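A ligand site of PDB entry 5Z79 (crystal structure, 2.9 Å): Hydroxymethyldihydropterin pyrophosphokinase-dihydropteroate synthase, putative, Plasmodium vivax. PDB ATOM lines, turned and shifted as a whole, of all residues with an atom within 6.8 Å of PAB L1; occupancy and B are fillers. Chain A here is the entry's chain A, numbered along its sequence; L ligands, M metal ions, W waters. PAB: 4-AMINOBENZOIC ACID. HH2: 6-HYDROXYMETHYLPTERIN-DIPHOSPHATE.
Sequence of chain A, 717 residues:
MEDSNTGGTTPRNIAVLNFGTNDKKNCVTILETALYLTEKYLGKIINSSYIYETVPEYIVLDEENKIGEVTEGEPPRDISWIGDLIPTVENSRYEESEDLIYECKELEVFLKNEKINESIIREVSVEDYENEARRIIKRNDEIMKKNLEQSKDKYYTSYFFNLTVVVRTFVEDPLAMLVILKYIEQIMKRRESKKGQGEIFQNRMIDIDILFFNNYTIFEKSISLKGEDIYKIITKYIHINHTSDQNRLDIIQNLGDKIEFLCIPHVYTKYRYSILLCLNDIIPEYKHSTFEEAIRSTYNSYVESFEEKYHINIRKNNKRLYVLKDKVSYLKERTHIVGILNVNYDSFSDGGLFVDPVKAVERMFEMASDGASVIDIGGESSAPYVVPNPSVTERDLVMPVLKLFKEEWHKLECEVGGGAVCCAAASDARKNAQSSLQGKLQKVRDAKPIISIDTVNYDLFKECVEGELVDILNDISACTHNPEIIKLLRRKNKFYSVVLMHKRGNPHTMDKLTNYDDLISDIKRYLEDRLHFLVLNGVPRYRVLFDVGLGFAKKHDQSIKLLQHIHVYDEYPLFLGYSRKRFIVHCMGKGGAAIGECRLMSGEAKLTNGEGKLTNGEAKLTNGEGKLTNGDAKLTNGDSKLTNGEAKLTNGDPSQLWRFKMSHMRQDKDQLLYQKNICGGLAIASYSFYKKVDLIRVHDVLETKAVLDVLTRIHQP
N of Arg 582 sits at hydrogen-bond distance from O1' of PAB L1 (2.8 Å). The guanidinium group (NE) of Arg 582 is in salt-bridge range of an oxygen (O2') of PAB L1 (2.6 Å). The backbone carbonyl oxygen (O) of Ser 382 lies within hydrogen-bond range of a nitrogen (N4) of PAB L1 (3.4 Å). O8 of HH2 L2 is in hydrogen-bond range of NZ of Lys 581, 2.7 Å away. N of Ser 382 lies within hydrogen-bond range of O6P of HH2 L2 (3.0 Å). The side-chain hydroxyl (OG) of Ser 381 lies within hydrogen-bond range of an oxygen (O5P) of HH2 L2, 2.5 Å away.
The guanidinium group of Arg 582 is in salt-bridge range of the side-chain carboxylate of Asp 511, at 2.9 Å. The backbone carbonyl oxygen (O) of Phe 552 lies close to the side-chain amino group (NZ) of Lys 554 (3.0 Å). NZ of Lys 581 lies within hydrogen-bond range of O of Leu 550, at 2.8 Å. OG of Ser 559 sits at hydrogen-bond distance from N of Gly 551, 3.1 Å away. N of Ala 383 sits at hydrogen-bond distance from OG of Ser 381.
Residues that only touch PAB L1: Phe 348 (3.3 Å), Ala 383 (3.6 Å), Pro 384 (3.7 Å), Gly 551 (3.6 Å), Phe 552 (3.1 Å) and Lys 581 (3.3 Å). Hydrophobic or aromatic side chains that line PAB L1: Phe 348, Ala 383, Pro 384 and Phe 552. Of the 21 residues printed, 8 come within 4 Å of PAB L1. Along chain A the residues within 4 Å of PAB L1 span positions 348 to 582. The nearest printed residue that does not touch PAB L1 is Leu 550 (4.5 Å).
Water W1 lies within hydrogen-bond range of an oxygen (O2') of PAB L1, the backbone NH (N) of Phe 583 and the backbone NH (N) of Arg 582.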
ATOM      1  N   PHE A 348      33.686 -25.239  13.369  1.00  0.00           N
ATOM      2  CA  PHE A 348      33.308 -26.503  12.724  1.00  0.00           C
ATOM      3  C   PHE A 348      34.190 -26.878  11.514  1.00  0.00           C
ATOM      4  O   PHE A 348      34.315 -28.061  11.208  1.00  0.00           O
ATOM      5  CB  PHE A 348      31.784 -26.607  12.441  1.00  0.00           C
ATOM      6  CG  PHE A 348      31.289 -25.720  11.339  1.00  0.00           C
ATOM      7  CD1 PHE A 348      31.361 -26.137  10.020  1.00  0.00           C
ATOM      8  CD2 PHE A 348      30.733 -24.485  11.621  1.00  0.00           C
ATOM      9  CE1 PHE A 348      30.907 -25.318   9.006  1.00  0.00           C
ATOM     10  CE2 PHE A 348      30.266 -23.671  10.624  1.00  0.00           C
ATOM     11  CZ  PHE A 348      30.345 -24.094   9.309  1.00  0.00           C
ATOM     12  N   SER A 381      32.498 -20.429  19.292  1.00  0.00           N
ATOM     13  CA  SER A 381      31.785 -21.027  18.182  1.00  0.00           C
ATOM     14  C   SER A 381      30.291 -21.112  18.513  1.00  0.00           C
ATOM     15  O   SER A 381      29.923 -21.357  19.660  1.00  0.00           O
ATOM     16  CB  SER A 381      32.380 -22.404  17.931  1.00  0.00           C
ATOM     17  OG  SER A 381      31.646 -23.133  16.969  1.00  0.00           O
ATOM     18  N   SER A 382      29.424 -20.903  17.513  1.00  0.00           N
ATOM     19  CA  SER A 382      27.989 -21.104  17.707  1.00  0.00           C
ATOM     20  C   SER A 382      27.412 -22.286  16.932  1.00  0.00           C
ATOM     21  O   SER A 382      26.182 -22.405  16.798  1.00  0.00           O
ATOM     22  CB  SER A 382      27.228 -19.836  17.344  1.00  0.00           C
ATOM     23  OG  SER A 382      27.404 -18.870  18.364  1.00  0.00           O
ATOM     24  N   ALA A 383      28.295 -23.167  16.469  1.00  0.00           N
ATOM     25  CA  ALA A 383      27.900 -24.262  15.593  1.00  0.00           C
ATOM     26  C   ALA A 383      27.141 -25.382  16.316  1.00  0.00           C
ATOM     27  O   ALA A 383      27.360 -25.593  17.494  1.00  0.00           O
ATOM     28  CB  ALA A 383      29.118 -24.820  14.880  1.00  0.00           C
ATOM     29  N   PRO A 384      26.288 -26.127  15.578  1.00  0.00           N
ATOM     30  CA  PRO A 384      25.357 -27.064  16.192  1.00  0.00           C
ATOM     31  C   PRO A 384      26.020 -28.030  17.153  1.00  0.00           C
ATOM     32  O   PRO A 384      27.047 -28.606  16.842  1.00  0.00           O
ATOM     33  CB  PRO A 384      24.750 -27.794  14.988  1.00  0.00           C
ATOM     34  CG  PRO A 384      24.793 -26.788  13.899  1.00  0.00           C
ATOM     35  CD  PRO A 384      26.131 -26.145  14.104  1.00  0.00           C
ATOM     36  N   ILE A 476      25.043 -11.950  17.254  1.00  0.00           N
ATOM     37  CA  ILE A 476      24.166 -12.946  16.675  1.00  0.00           C
ATOM     38  C   ILE A 476      22.839 -13.062  17.421  1.00  0.00           C
ATOM     39  O   ILE A 476      21.956 -13.780  16.960  1.00  0.00           O
ATOM     40  CB  ILE A 476      24.860 -14.325  16.550  1.00  0.00           C
ATOM     41  CG1 ILE A 476      25.384 -14.805  17.899  1.00  0.00           C
ATOM     42  CG2 ILE A 476      26.021 -14.224  15.536  1.00  0.00           C
ATOM     43  CD1 ILE A 476      25.686 -16.280  17.911  1.00  0.00           C
ATOM     44  N   MET A 510      18.936 -24.954  19.153  1.00  0.00           N
ATOM     45  CA  MET A 510      18.458 -24.168  17.993  1.00  0.00           C
ATOM     46  C   MET A 510      17.721 -25.118  17.054  1.00  0.00           C
ATOM     47  O   MET A 510      16.564 -24.877  16.714  1.00  0.00           O
ATOM     48  CB  MET A 510      19.577 -23.357  17.294  1.00  0.00           C
ATOM     49  CG  MET A 510      20.744 -24.142  16.694  1.00  0.00           C
ATOM     50  SD  MET A 510      21.999 -23.178  15.751  1.00  0.00           S
ATOM     51  CE  MET A 510      22.663 -22.070  17.012  1.00  0.00           C
ATOM     52  N   ASP A 511      18.343 -26.245  16.721  1.00  0.00           N
ATOM     53  CA  ASP A 511      17.772 -27.182  15.759  1.00  0.00           C
ATOM     54  C   ASP A 511      16.372 -27.650  16.104  1.00  0.00           C
ATOM     55  O   ASP A 511      15.637 -28.088  15.238  1.00  0.00           O
ATOM     56  CB  ASP A 511      18.725 -28.372  15.562  1.00  0.00           C
ATOM     57  CG  ASP A 511      19.902 -28.055  14.574  1.00  0.00           C
ATOM     58  OD1 ASP A 511      19.853 -27.070  13.787  1.00  0.00           O
ATOM     59  OD2 ASP A 511      20.883 -28.845  14.582  1.00  0.00           O
ATOM     60  N   LEU A 550      21.177 -17.748   8.564  1.00  0.00           N
ATOM     61  CA  LEU A 550      20.977 -19.014   7.935  1.00  0.00           C
ATOM     62  C   LEU A 550      21.536 -20.155   8.756  1.00  0.00           C
ATOM     63  O   LEU A 550      22.634 -20.104   9.202  1.00  0.00           O
ATOM     64  CB  LEU A 550      21.579 -18.973   6.536  1.00  0.00           C
ATOM     65  CG  LEU A 550      20.992 -17.994   5.549  1.00  0.00           C
ATOM     66  CD1 LEU A 550      21.939 -17.755   4.415  1.00  0.00           C
ATOM     67  CD2 LEU A 550      19.686 -18.499   5.018  1.00  0.00           C
ATOM     68  N   GLY A 551      20.758 -21.208   8.892  1.00  0.00           N
ATOM     69  CA  GLY A 551      21.130 -22.383   9.654  1.00  0.00           C
ATOM     70  C   GLY A 551      20.895 -22.285  11.149  1.00  0.00           C
ATOM     71  O   GLY A 551      21.012 -23.286  11.824  1.00  0.00           O
ATOM     72  N   PHE A 552      20.576 -21.101  11.670  1.00  0.00           N
ATOM     73  CA  PHE A 552      20.344 -20.901  13.122  1.00  0.00           C
ATOM     74  C   PHE A 552      18.868 -20.998  13.451  1.00  0.00           C
ATOM     75  O   PHE A 552      18.131 -20.037  13.314  1.00  0.00           O
ATOM     76  CB  PHE A 552      20.792 -19.518  13.555  1.00  0.00           C
ATOM     77  CG  PHE A 552      22.276 -19.338  13.674  1.00  0.00           C
ATOM     78  CD1 PHE A 552      23.031 -18.951  12.588  1.00  0.00           C
ATOM     79  CD2 PHE A 552      22.903 -19.478  14.896  1.00  0.00           C
ATOM     80  CE1 PHE A 552      24.393 -18.734  12.688  1.00  0.00           C
ATOM     81  CE2 PHE A 552      24.270 -19.256  15.019  1.00  0.00           C
ATOM     82  CZ  PHE A 552      25.014 -18.882  13.908  1.00  0.00           C
ATOM     83  N   ALA A 553      18.430 -22.148  13.903  1.00  0.00           N
ATOM     84  CA  ALA A 553      17.020 -22.351  14.237  1.00  0.00           C
ATOM     85  C   ALA A 553      16.132 -22.286  12.996  1.00  0.00           C
ATOM     86  O   ALA A 553      15.023 -21.742  13.009  1.00  0.00           O
ATOM     87  CB  ALA A 553      16.574 -21.371  15.292  1.00  0.00           C
ATOM     88  N   LYS A 554      16.678 -22.867  11.914  1.00  0.00           N
ATOM     89  CA  LYS A 554      15.959 -23.175  10.684  1.00  0.00           C
ATOM     90  C   LYS A 554      16.302 -24.575  10.196  1.00  0.00           C
ATOM     91  O   LYS A 554      17.485 -24.977  10.197  1.00  0.00           O
ATOM     92  CB  LYS A 554      16.335 -22.169   9.629  1.00  0.00           C
ATOM     93  CG  LYS A 554      15.874 -20.770   9.941  1.00  0.00           C
ATOM     94  CD  LYS A 554      16.982 -19.964  10.578  1.00  0.00           C
ATOM     95  CE  LYS A 554      16.527 -18.535  10.900  1.00  0.00           C
ATOM     96  NZ  LYS A 554      17.583 -17.690  11.511  1.00  0.00           N
ATOM     97  N   HIS A 556      16.730 -27.065   7.012  1.00  0.00           N
ATOM     98  CA  HIS A 556      17.322 -26.791   5.723  1.00  0.00           C
ATOM     99  C   HIS A 556      16.384 -26.212   4.611  1.00  0.00           C
ATOM    100  O   HIS A 556      16.747 -25.246   3.944  1.00  0.00           O
ATOM    101  CB  HIS A 556      17.984 -28.071   5.261  1.00  0.00           C
ATOM    102  CG  HIS A 556      19.108 -28.519   6.129  1.00  0.00           C
ATOM    103  ND1 HIS A 556      19.816 -27.638   6.935  1.00  0.00           N
ATOM    104  CD2 HIS A 556      19.675 -29.732   6.281  1.00  0.00           C
ATOM    105  CE1 HIS A 556      20.761 -28.317   7.564  1.00  0.00           C
ATOM    106  NE2 HIS A 556      20.703 -29.582   7.174  1.00  0.00           N
ATOM    107  N   SER A 559      16.013 -22.485   5.467  1.00  0.00           N
ATOM    108  CA  SER A 559      17.153 -21.644   5.108  1.00  0.00           C
ATOM    109  C   SER A 559      17.029 -21.295   3.639  1.00  0.00           C
ATOM    110  O   SER A 559      17.181 -20.144   3.257  1.00  0.00           O
ATOM    111  CB  SER A 559      18.497 -22.336   5.409  1.00  0.00           C
ATOM    112  OG  SER A 559      18.751 -22.433   6.805  1.00  0.00           O
ATOM    113  N   TYR A 578      26.250 -17.785   4.510  1.00  0.00           N
ATOM    114  CA  TYR A 578      25.927 -19.159   4.169  1.00  0.00           C
ATOM    115  C   TYR A 578      27.117 -20.103   4.340  1.00  0.00           C
ATOM    116  O   TYR A 578      26.944 -21.318   4.440  1.00  0.00           O
ATOM    117  CB  TYR A 578      25.517 -19.215   2.718  1.00  0.00           C
ATOM    118  CG  TYR A 578      26.531 -18.624   1.776  1.00  0.00           C
ATOM    119  CD1 TYR A 578      27.650 -19.330   1.429  1.00  0.00           C
ATOM    120  CD2 TYR A 578      26.359 -17.362   1.234  1.00  0.00           C
ATOM    121  CE1 TYR A 578      28.579 -18.816   0.570  1.00  0.00           C
ATOM    122  CE2 TYR A 578      27.285 -16.821   0.371  1.00  0.00           C
ATOM    123  CZ  TYR A 578      28.393 -17.570   0.035  1.00  0.00           C
ATOM    124  OH  TYR A 578      29.348 -17.098  -0.830  1.00  0.00           O
ATOM    125  N   SER A 579      28.308 -19.525   4.354  1.00  0.00           N
ATOM    126  CA  SER A 579      29.532 -20.268   4.096  1.00  0.00           C
ATOM    127  C   SER A 579      29.755 -21.534   4.917  1.00  0.00           C
ATOM    128  O   SER A 579      29.710 -21.548   6.143  1.00  0.00           O
ATOM    129  CB  SER A 579      30.727 -19.358   4.237  1.00  0.00           C
ATOM    130  OG  SER A 579      31.864 -20.112   4.032  1.00  0.00           O
ATOM    131  N   ARG A 580      30.007 -22.600   4.163  1.00  0.00           N
ATOM    132  CA  ARG A 580      30.191 -23.971   4.646  1.00  0.00           C
ATOM    133  C   ARG A 580      29.059 -24.574   5.478  1.00  0.00           C
ATOM    134  O   ARG A 580      29.241 -25.690   5.976  1.00  0.00           O
ATOM    135  CB  ARG A 580      31.522 -24.100   5.387  1.00  0.00           C
ATOM    136  CG  ARG A 580      32.691 -23.713   4.528  1.00  0.00           C
ATOM    137  CD  ARG A 580      33.989 -23.965   5.259  1.00  0.00           C
ATOM    138  NE  ARG A 580      35.126 -23.690   4.401  1.00  0.00           N
ATOM    139  CZ  ARG A 580      36.376 -23.544   4.820  1.00  0.00           C
ATOM    140  NH1 ARG A 580      36.674 -23.654   6.105  1.00  0.00           N
ATOM    141  NH2 ARG A 580      37.330 -23.279   3.966  1.00  0.00           N
ATOM    142  N   LYS A 581      27.910 -23.900   5.612  1.00  0.00           N
ATOM    143  CA  LYS A 581      26.793 -24.435   6.410  1.00  0.00           C
ATOM    144  C   LYS A 581      26.200 -25.706   5.811  1.00  0.00           C
ATOM    145  O   LYS A 581      26.489 -26.055   4.678  1.00  0.00           O
ATOM    146  CB  LYS A 581      25.718 -23.387   6.640  1.00  0.00           C
ATOM    147  CG  LYS A 581      26.326 -22.211   7.395  1.00  0.00           C
ATOM    148  CD  LYS A 581      25.335 -21.248   8.045  1.00  0.00           C
ATOM    149  CE  LYS A 581      26.112 -20.204   8.827  1.00  0.00           C
ATOM    150  NZ  LYS A 581      25.278 -19.063   9.292  1.00  0.00           N
ATOM    151  N   ARG A 582      25.413 -26.419   6.619  1.00  0.00           N
ATOM    152  CA  ARG A 582      24.912 -27.767   6.269  1.00  0.00           C
ATOM    153  C   ARG A 582      23.931 -27.793   5.078  1.00  0.00           C
ATOM    154  O   ARG A 582      23.901 -28.755   4.266  1.00  0.00           O
ATOM    155  CB  ARG A 582      24.194 -28.405   7.473  1.00  0.00           C
ATOM    156  CG  ARG A 582      25.032 -28.761   8.694  1.00  0.00           C
ATOM    157  CD  ARG A 582      24.110 -29.049   9.866  1.00  0.00           C
ATOM    158  NE  ARG A 582      23.406 -27.852  10.342  1.00  0.00           N
ATOM    159  CZ  ARG A 582      22.753 -27.746  11.489  1.00  0.00           C
ATOM    160  NH1 ARG A 582      22.701 -28.756  12.336  1.00  0.00           N
ATOM    161  NH2 ARG A 582      22.168 -26.594  11.812  1.00  0.00           N
ATOM    162  N   PHE A 583      23.118 -26.730   5.008  1.00  0.00           N
ATOM    163  CA  PHE A 583      21.955 -26.657   4.134  1.00  0.00           C
ATOM    164  C   PHE A 583      22.386 -26.617   2.700  1.00  0.00           C
ATOM    165  O   PHE A 583      21.613 -26.954   1.819  1.00  0.00           O
ATOM    166  CB  PHE A 583      21.093 -25.404   4.467  1.00  0.00           C
ATOM    167  CG  PHE A 583      21.635 -24.113   3.910  1.00  0.00           C
ATOM    168  CD1 PHE A 583      22.556 -23.372   4.610  1.00  0.00           C
ATOM    169  CD2 PHE A 583      21.200 -23.651   2.684  1.00  0.00           C
ATOM    170  CE1 PHE A 583      23.055 -22.194   4.103  1.00  0.00           C
ATOM    171  CE2 PHE A 583      21.695 -22.468   2.164  1.00  0.00           C
ATOM    172  CZ  PHE A 583      22.633 -21.730   2.882  1.00  0.00           C
HETATM  173  C1' PAB L   1      24.899 -25.056  10.056  1.00  0.00           C
HETATM  174  O1' PAB L   1      25.689 -25.631   9.285  1.00  0.00           O
HETATM  175  O2' PAB L   1      23.681 -25.328  10.073  1.00  0.00           O
HETATM  176  C1  PAB L   1      25.440 -24.049  11.020  1.00  0.00           C
HETATM  177  C2  PAB L   1      26.814 -23.949  11.191  1.00  0.00           C
HETATM  178  C3  PAB L   1      27.330 -23.024  12.079  1.00  0.00           C
HETATM  179  C4  PAB L   1      26.472 -22.199  12.796  1.00  0.00           C
HETATM  180  C5  PAB L   1      25.100 -22.290  12.636  1.00  0.00           C
HETATM  181  C6  PAB L   1      24.588 -23.216  11.738  1.00  0.00           C
HETATM  182  N4  PAB L   1      26.997 -21.312  13.660  1.00  0.00           N
HETATM  183  N1  HH2 L   2      27.397 -17.593  11.277  1.00  0.00           N
HETATM  184  C2  HH2 L   2      28.437 -18.004  12.043  1.00  0.00           C
HETATM  185  C3  HH2 L   2      29.149 -17.098  12.826  1.00  0.00           C
HETATM  186  N4  HH2 L   2      28.843 -15.798  12.854  1.00  0.00           N
HETATM  187  N5  HH2 L   2      27.495 -14.023  12.107  1.00  0.00           N
HETATM  188  C6  HH2 L   2      26.461 -13.580  11.350  1.00  0.00           C
HETATM  189  N6  HH2 L   2      26.150 -12.265  11.385  1.00  0.00           N
HETATM  190  N7  HH2 L   2      25.730 -14.401  10.572  1.00  0.00           N
HETATM  191  C8  HH2 L   2      25.952 -15.718  10.470  1.00  0.00           C
HETATM  192  O8  HH2 L   2      25.247 -16.438   9.712  1.00  0.00           O
HETATM  193  C9  HH2 L   2      27.063 -16.280  11.270  1.00  0.00           C
HETATM  194  C10 HH2 L   2      27.829 -15.335  12.114  1.00  0.00           C
HETATM  195  C11 HH2 L   2      28.874 -19.458  12.030  1.00  0.00           C
HETATM  196  O4  HH2 L   2      29.997 -19.628  11.118  1.00  0.00           O
HETATM  197  P1  HH2 L   2      31.541 -19.926  11.540  1.00  0.00           P
HETATM  198  O1P HH2 L   2      32.306 -20.576  10.422  1.00  0.00           O
HETATM  199  O2P HH2 L   2      32.185 -18.744  12.255  1.00  0.00           O
HETATM  200  O3P HH2 L   2      31.288 -21.115  12.609  1.00  0.00           O
HETATM  201  P2  HH2 L   2      31.507 -20.975  14.202  1.00  0.00           P
HETATM  202  O4P HH2 L   2      32.758 -20.116  14.425  1.00  0.00           O
HETATM  203  O5P HH2 L   2      31.567 -22.439  14.572  1.00  0.00           O
HETATM  204  O6P HH2 L   2      30.274 -20.265  14.709  1.00  0.00           O
HETATM  205 MG    MG M   1      32.848 -17.936  14.197  1.00  0.00          MG
HETATM  206  O   HOH W   1      22.353 -25.054   7.611  1.00  0.00           O
